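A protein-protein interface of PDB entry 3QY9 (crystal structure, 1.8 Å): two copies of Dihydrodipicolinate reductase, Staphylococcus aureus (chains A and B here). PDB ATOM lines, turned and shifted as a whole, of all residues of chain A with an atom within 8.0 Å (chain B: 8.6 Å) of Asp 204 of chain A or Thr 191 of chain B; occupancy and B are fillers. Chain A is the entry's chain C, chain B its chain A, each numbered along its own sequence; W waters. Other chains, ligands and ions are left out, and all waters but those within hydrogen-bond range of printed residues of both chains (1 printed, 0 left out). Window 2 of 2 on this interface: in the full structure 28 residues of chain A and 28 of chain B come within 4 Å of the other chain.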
ATOM      1  N   PHE A 130       2.764 -28.530 -26.445  1.00  0.00           N
ATOM      2  CA  PHE A 130       3.854 -27.684 -25.965  1.00  0.00           C
ATOM      3  C   PHE A 130       5.181 -28.141 -26.557  1.00  0.00           C
ATOM      4  O   PHE A 130       5.397 -29.338 -26.740  1.00  0.00           O
ATOM      5  CB  PHE A 130       3.949 -27.789 -24.439  1.00  0.00           C
ATOM      6  CG  PHE A 130       2.857 -27.058 -23.693  1.00  0.00           C
ATOM      7  CD1 PHE A 130       3.189 -26.065 -22.774  1.00  0.00           C
ATOM      8  CD2 PHE A 130       1.512 -27.377 -23.878  1.00  0.00           C
ATOM      9  CE1 PHE A 130       2.197 -25.384 -22.060  1.00  0.00           C
ATOM     10  CE2 PHE A 130       0.511 -26.700 -23.167  1.00  0.00           C
ATOM     11  CZ  PHE A 130       0.862 -25.701 -22.253  1.00  0.00           C
ATOM     12  N   ASP A 131       6.061 -27.187 -26.849  1.00  0.00           N
ATOM     13  CA  ASP A 131       7.439 -27.479 -27.261  1.00  0.00           C
ATOM     14  C   ASP A 131       8.261 -27.924 -26.061  1.00  0.00           C
ATOM     15  O   ASP A 131       8.188 -27.311 -24.993  1.00  0.00           O
ATOM     16  CB  ASP A 131       8.095 -26.237 -27.872  1.00  0.00           C
ATOM     17  CG  ASP A 131       7.435 -25.797 -29.167  1.00  0.00           C
ATOM     18  OD1 ASP A 131       6.857 -26.652 -29.871  1.00  0.00           O
ATOM     19  OD2 ASP A 131       7.503 -24.593 -29.487  1.00  0.00           O
ATOM     20  N   ALA A 201       6.948 -25.413 -23.476  1.00  0.00           N
ATOM     21  CA  ALA A 201       6.618 -24.040 -23.851  1.00  0.00           C
ATOM     22  C   ALA A 201       5.393 -24.006 -24.754  1.00  0.00           C
ATOM     23  O   ALA A 201       5.409 -24.527 -25.871  1.00  0.00           O
ATOM     24  CB  ALA A 201       7.819 -23.352 -24.514  1.00  0.00           C
ATOM     25  N   GLY A 202       4.321 -23.402 -24.256  1.00  0.00           N
ATOM     26  CA  GLY A 202       3.090 -23.295 -25.025  1.00  0.00           C
ATOM     27  C   GLY A 202       2.793 -21.861 -25.427  1.00  0.00           C
ATOM     28  O   GLY A 202       3.688 -21.011 -25.474  1.00  0.00           O
ATOM     29  N   THR A 203       1.525 -21.592 -25.697  1.00  0.00           N
ATOM     30  CA  THR A 203       1.100 -20.260 -26.108  1.00  0.00           C
ATOM     31  C   THR A 203       0.973 -19.338 -24.897  1.00  0.00           C
ATOM     32  O   THR A 203      -0.002 -19.399 -24.144  1.00  0.00           O
ATOM     33  CB  THR A 203      -0.191 -20.335 -26.949  1.00  0.00           C
ATOM     34  OG1 THR A 203       0.073 -21.157 -28.091  1.00  0.00           O
ATOM     35  CG2 THR A 203      -0.638 -18.949 -27.428  1.00  0.00           C
ATOM     36  N   ASP A 204       1.990 -18.493 -24.720  1.00  0.00           N
ATOM     37  CA  ASP A 204       2.044 -17.520 -23.628  1.00  0.00           C
ATOM     38  C   ASP A 204       2.082 -18.147 -22.234  1.00  0.00           C
ATOM     39  O   ASP A 204       1.802 -17.481 -21.240  1.00  0.00           O
ATOM     40  CB  ASP A 204       0.907 -16.496 -23.749  1.00  0.00           C
ATOM     41  CG  ASP A 204       1.214 -15.395 -24.752  1.00  0.00           C
ATOM     42  OD1 ASP A 204       2.023 -15.615 -25.687  1.00  0.00           O
ATOM     43  OD2 ASP A 204       0.643 -14.297 -24.597  1.00  0.00           O
ATOM     44  N   GLU A 205       2.443 -19.425 -22.168  1.00  0.00           N
ATOM     45  CA  GLU A 205       2.646 -20.099 -20.890  1.00  0.00           C
ATOM     46  C   GLU A 205       3.713 -21.183 -20.994  1.00  0.00           C
ATOM     47  O   GLU A 205       3.867 -21.834 -22.030  1.00  0.00           O
ATOM     48  CB  GLU A 205       1.337 -20.659 -20.319  1.00  0.00           C
ATOM     49  CG  GLU A 205       0.604 -21.663 -21.208  1.00  0.00           C
ATOM     50  CD  GLU A 205      -0.765 -22.045 -20.663  1.00  0.00           C
ATOM     51  OE1 GLU A 205      -1.044 -21.780 -19.473  1.00  0.00           O
ATOM     52  OE2 GLU A 205      -1.576 -22.604 -21.433  1.00  0.00           O
ATOM     53  N   THR A 206       4.465 -21.350 -19.917  1.00  0.00           N
ATOM     54  CA  THR A 206       5.451 -22.408 -19.854  1.00  0.00           C
ATOM     55  C   THR A 206       5.238 -23.206 -18.583  1.00  0.00           C
ATOM     56  O   THR A 206       4.755 -22.675 -17.583  1.00  0.00           O
ATOM     57  CB  THR A 206       6.885 -21.847 -19.844  1.00  0.00           C
ATOM     58  OG1 THR A 206       7.055 -21.005 -18.698  1.00  0.00           O
ATOM     59  CG2 THR A 206       7.173 -21.035 -21.112  1.00  0.00           C
ATOM     60  N   ALA B 137      16.534 -17.814 -24.169  1.00  0.00           N
ATOM     61  CA  ALA B 137      15.336 -18.518 -24.612  1.00  0.00           C
ATOM     62  C   ALA B 137      14.462 -17.562 -25.390  1.00  0.00           C
ATOM     63  O   ALA B 137      14.264 -16.422 -24.974  1.00  0.00           O
ATOM     64  CB  ALA B 137      14.557 -19.071 -23.409  1.00  0.00           C
ATOM     65  N   HIS B 138      13.933 -18.034 -26.521  1.00  0.00           N
ATOM     66  CA  HIS B 138      13.038 -17.238 -27.347  1.00  0.00           C
ATOM     67  C   HIS B 138      11.970 -18.141 -27.931  1.00  0.00           C
ATOM     68  O   HIS B 138      12.092 -19.366 -27.878  1.00  0.00           O
ATOM     69  CB  HIS B 138      13.807 -16.512 -28.461  1.00  0.00           C
ATOM     70  CG  HIS B 138      14.554 -15.307 -27.979  1.00  0.00           C
ATOM     71  ND1 HIS B 138      15.773 -15.399 -27.341  1.00  0.00           N
ATOM     72  CD2 HIS B 138      14.235 -13.992 -27.990  1.00  0.00           C
ATOM     73  CE1 HIS B 138      16.185 -14.193 -26.998  1.00  0.00           C
ATOM     74  NE2 HIS B 138      15.266 -13.320 -27.375  1.00  0.00           N
ATOM     75  N   HIS B 139      10.924 -17.517 -28.460  1.00  0.00           N
ATOM     76  CA  HIS B 139       9.806 -18.199 -29.114  1.00  0.00           C
ATOM     77  C   HIS B 139      10.220 -19.129 -30.271  1.00  0.00           C
ATOM     78  O   HIS B 139      11.343 -19.038 -30.781  1.00  0.00           O
ATOM     79  CB  HIS B 139       8.812 -17.145 -29.622  1.00  0.00           C
ATOM     80  CG  HIS B 139       9.420 -16.146 -30.558  1.00  0.00           C
ATOM     81  ND1 HIS B 139       9.612 -16.407 -31.896  1.00  0.00           N
ATOM     82  CD2 HIS B 139       9.878 -14.889 -30.350  1.00  0.00           C
ATOM     83  CE1 HIS B 139      10.161 -15.354 -32.475  1.00  0.00           C
ATOM     84  NE2 HIS B 139      10.333 -14.418 -31.558  1.00  0.00           N
ATOM     85  N   ASN B 140       9.304 -20.011 -30.689  1.00  0.00           N
ATOM     86  CA  ASN B 140       9.622 -21.028 -31.696  1.00  0.00           C
ATOM     87  C   ASN B 140       9.711 -20.529 -33.144  1.00  0.00           C
ATOM     88  O   ASN B 140       9.974 -21.324 -34.042  1.00  0.00           O
ATOM     89  CB  ASN B 140       8.676 -22.244 -31.600  1.00  0.00           C
ATOM     90  CG  ASN B 140       7.214 -21.889 -31.851  1.00  0.00           C
ATOM     91  OD1 ASN B 140       6.895 -20.870 -32.466  1.00  0.00           O
ATOM     92  ND2 ASN B 140       6.314 -22.742 -31.364  1.00  0.00           N
ATOM     93  N   LYS B 141       9.504 -19.228 -33.361  1.00  0.00           N
ATOM     94  CA  LYS B 141       9.620 -18.640 -34.705  1.00  0.00           C
ATOM     95  C   LYS B 141      11.000 -18.044 -34.983  1.00  0.00           C
ATOM     96  O   LYS B 141      11.322 -17.740 -36.138  1.00  0.00           O
ATOM     97  CB  LYS B 141       8.539 -17.582 -34.933  1.00  0.00           C
ATOM     98  CG  LYS B 141       7.136 -18.153 -35.051  1.00  0.00           C
ATOM     99  CD  LYS B 141       6.096 -17.041 -35.148  1.00  0.00           C
ATOM    100  CE  LYS B 141       4.676 -17.576 -34.971  1.00  0.00           C
ATOM    101  NZ  LYS B 141       4.342 -18.659 -35.941  1.00  0.00           N
ATOM    102  N   ARG B 188      14.621 -22.698 -27.722  1.00  0.00           N
ATOM    103  CA  ARG B 188      13.526 -22.232 -28.570  1.00  0.00           C
ATOM    104  C   ARG B 188      12.241 -22.958 -28.219  1.00  0.00           C
ATOM    105  O   ARG B 188      12.218 -24.185 -28.127  1.00  0.00           O
ATOM    106  CB  ARG B 188      13.855 -22.441 -30.058  1.00  0.00           C
ATOM    107  CG  ARG B 188      15.056 -21.619 -30.546  1.00  0.00           C
ATOM    108  CD  ARG B 188      14.714 -20.146 -30.722  1.00  0.00           C
ATOM    109  NE  ARG B 188      15.898 -19.360 -31.071  1.00  0.00           N
ATOM    110  CZ  ARG B 188      16.725 -18.806 -30.185  1.00  0.00           C
ATOM    111  NH1 ARG B 188      16.516 -18.948 -28.875  1.00  0.00           N
ATOM    112  NH2 ARG B 188      17.776 -18.116 -30.609  1.00  0.00           N
ATOM    113  N   GLY B 189      11.167 -22.205 -28.014  1.00  0.00           N
ATOM    114  CA  GLY B 189       9.875 -22.831 -27.796  1.00  0.00           C
ATOM    115  C   GLY B 189       8.764 -21.853 -27.515  1.00  0.00           C
ATOM    116  O   GLY B 189       8.995 -20.766 -26.981  1.00  0.00           O
ATOM    117  N   GLY B 190       7.552 -22.266 -27.869  1.00  0.00           N
ATOM    118  CA  GLY B 190       6.350 -21.498 -27.599  1.00  0.00           C
ATOM    119  C   GLY B 190       6.440 -20.068 -28.089  1.00  0.00           C
ATOM    120  O   GLY B 190       6.902 -19.807 -29.206  1.00  0.00           O
ATOM    121  N   THR B 191       6.006 -19.145 -27.240  1.00  0.00           N
ATOM    122  CA  THR B 191       5.914 -17.732 -27.614  1.00  0.00           C
ATOM    123  C   THR B 191       6.825 -16.859 -26.746  1.00  0.00           C
ATOM    124  O   THR B 191       6.646 -15.635 -26.681  1.00  0.00           O
ATOM    125  CB  THR B 191       4.471 -17.212 -27.495  1.00  0.00           C
ATOM    126  OG1 THR B 191       4.037 -17.332 -26.133  1.00  0.00           O
ATOM    127  CG2 THR B 191       3.517 -17.976 -28.426  1.00  0.00           C
ATOM    128  N   ILE B 192       7.799 -17.495 -26.096  1.00  0.00           N
ATOM    129  CA  ILE B 192       8.720 -16.831 -25.159  1.00  0.00           C
ATOM    130  C   ILE B 192       9.251 -15.533 -25.764  1.00  0.00           C
ATOM    131  O   ILE B 192       9.861 -15.544 -26.828  1.00  0.00           O
ATOM    132  CB  ILE B 192       9.883 -17.769 -24.754  1.00  0.00           C
ATOM    133  CG1 ILE B 192       9.341 -18.973 -23.963  1.00  0.00           C
ATOM    134  CG2 ILE B 192      10.948 -17.018 -23.928  1.00  0.00           C
ATOM    135  CD1 ILE B 192      10.336 -20.109 -23.815  1.00  0.00           C
ATOM    136  N   VAL B 193       8.993 -14.409 -25.096  1.00  0.00           N
ATOM    137  CA  VAL B 193       9.383 -13.106 -25.650  1.00  0.00           C
ATOM    138  C   VAL B 193      10.908 -12.947 -25.655  1.00  0.00           C
ATOM    139  O   VAL B 193      11.489 -12.453 -26.629  1.00  0.00           O
ATOM    140  CB  VAL B 193       8.678 -11.939 -24.925  1.00  0.00           C
ATOM    141  CG1 VAL B 193       9.247 -10.582 -25.365  1.00  0.00           C
ATOM    142  CG2 VAL B 193       7.180 -11.988 -25.221  1.00  0.00           C
ATOM    143  N   GLY B 194      11.550 -13.393 -24.582  1.00  0.00           N
ATOM    144  CA  GLY B 194      13.005 -13.358 -24.503  1.00  0.00           C
ATOM    145  C   GLY B 194      13.506 -13.385 -23.076  1.00  0.00           C
ATOM    146  O   GLY B 194      13.161 -12.529 -22.265  1.00  0.00           O
ATOM    147  N   ALA B 213      11.826 -10.804 -20.422  1.00  0.00           N
ATOM    148  CA  ALA B 213      10.915  -9.871 -21.068  1.00  0.00           C
ATOM    149  C   ALA B 213       9.537 -10.507 -21.192  1.00  0.00           C
ATOM    150  O   ALA B 213       9.413 -11.665 -21.589  1.00  0.00           O
ATOM    151  CB  ALA B 213      11.438  -9.485 -22.442  1.00  0.00           C
ATOM    152  N   GLN B 214       8.514  -9.728 -20.859  1.00  0.00           N
ATOM    153  CA  GLN B 214       7.122 -10.172 -20.901  1.00  0.00           C
ATOM    154  C   GLN B 214       6.413  -9.682 -22.174  1.00  0.00           C
ATOM    155  O   GLN B 214       5.404 -10.258 -22.590  1.00  0.00           O
ATOM    156  CB  GLN B 214       6.404  -9.631 -19.667  1.00  0.00           C
ATOM    157  CG  GLN B 214       5.037 -10.233 -19.362  1.00  0.00           C
ATOM    158  CD  GLN B 214       4.625  -9.967 -17.926  1.00  0.00           C
ATOM    159  OE1 GLN B 214       4.600 -10.879 -17.090  1.00  0.00           O
ATOM    160  NE2 GLN B 214       4.330  -8.707 -17.623  1.00  0.00           N
ATOM    161  N   SER B 215       6.953  -8.624 -22.779  1.00  0.00           N
ATOM    162  CA  SER B 215       6.366  -7.977 -23.950  1.00  0.00           C
ATOM    163  C   SER B 215       7.439  -7.227 -24.722  1.00  0.00           C
ATOM    164  O   SER B 215       8.383  -6.710 -24.128  1.00  0.00           O
ATOM    165  CB  SER B 215       5.277  -6.985 -23.512  1.00  0.00           C
ATOM    166  OG  SER B 215       4.794  -6.233 -24.614  1.00  0.00           O
ATOM    167  N   LYS B 216       7.286  -7.148 -26.041  1.00  0.00           N
ATOM    168  CA  LYS B 216       8.178  -6.310 -26.852  1.00  0.00           C
ATOM    169  C   LYS B 216       7.974  -4.809 -26.596  1.00  0.00           C
ATOM    170  O   LYS B 216       8.725  -3.972 -27.112  1.00  0.00           O
ATOM    171  CB  LYS B 216       8.066  -6.666 -28.340  1.00  0.00           C
ATOM    172  CG  LYS B 216       8.806  -7.959 -28.695  1.00  0.00           C
ATOM    173  CD  LYS B 216       8.610  -8.376 -30.154  1.00  0.00           C
ATOM    174  CE  LYS B 216       9.578  -7.656 -31.082  1.00  0.00           C
ATOM    175  NZ  LYS B 216       9.406  -8.080 -32.501  1.00  0.00           N
HETATM  176  O   HOH W   1       5.888 -19.908 -24.360  1.00  0.00           O
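No position is printed for both chains.
Among the printed residues, merely in contact across the chains: Asp 131 of chain A with Gly 189 of chain B (3.4 Å), Ala 201 of chain A with Gly 189 of chain B (3.5 Å), Ala 201 of chain A with Gly 190 of chain B (3.5 Å), Gly 202 of chain A with Gly 190 of chain B (3.4 Å) and Thr 203 of chain A with Thr 191 of chain B (3.9 Å).
Water W1 lies within hydrogen-bond range of O of Gly 202 of chain A (2.7 Å) and N of Thr 191 of chain B (3.0 Å).
Of the 8 printed residues of chain A, 5 touch a printed residue of chain B. Printed residues of chain A that touch a printed residue of chain B: Asp 131, Ala 201, Gly 202, Thr 203 and Asp 204. Among the printed residues, no Asp or Glu carboxylate lies within 4 Å of a Lys or Arg side-chain nitrogen of the other chain.
OD2 of Asp 131 of chain A is in hydrogen-bond range of ND2 of Asn 140 of chain B, 2.9 Å away. N of Gly 190 of chain B lies within hydrogen-bond range of OD2 of Asp 131 of chain A, 2.8 Å away. The backbone carbonyl oxygen (O) of Gly 202 of chain A lies within hydrogen-bond range of the backbone NH (N) of Thr 191 of chain B (3.5 Å). The side-chain hydroxyl (OG1) of Thr 191 of chain B sits at hydrogen-bond distance from the side-chain carboxylate (OD1) of Asp 204 of chain A (2.7 Å).
The backbone carbonyl oxygen (O) of His 138 of chain B sits at hydrogen-bond distance from the backbone NH (N) of Gly 189 of chain B. The backbone NH of Asn 140 of chain B is in hydrogen-bond range of the backbone carbonyl oxygen of Gly 190 of chain B (2.8 Å). N of Ala 201 of chain A sits at hydrogen-bond distance from O of Asp 131 of chain A (2.7 Å).
Of the printed residues of chain B, Asp 131 of chain A touches Asn 140 (2.9 Å), Gly 189 (3.4 Å) and Gly 190 (2.8 Å). Of the printed residues of chain B, Ala 201 of chain A touches Gly 189 (3.5 Å) and Gly 190 (3.5 Å). Of the printed residues of chain B, Asp 204 of chain A touches Thr 191. Printed residues of chain A within 4 Å of Gly 189 of chain B: Asp 131 (3.4 Å) and Ala 201 (3.5 Å). Of chain A, only Gly 202, Thr 203 and Asp 204 come within 4 Å of Thr 191 of chain B. Lys 216 of chain B touches none of the printed residues of chain A. The nearest residue of chain B that does not touch Asp 204 of chain A is Gly 190 of chain B (5.8 Å). The nearest residue of chain A that does not touch Thr 191 of chain B is Glu 205 of chain A (4.8 Å). The nearest printed residue of chain B that does not touch Thr 203 of chain A is Gly 190 of chain B (5.2 Å).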
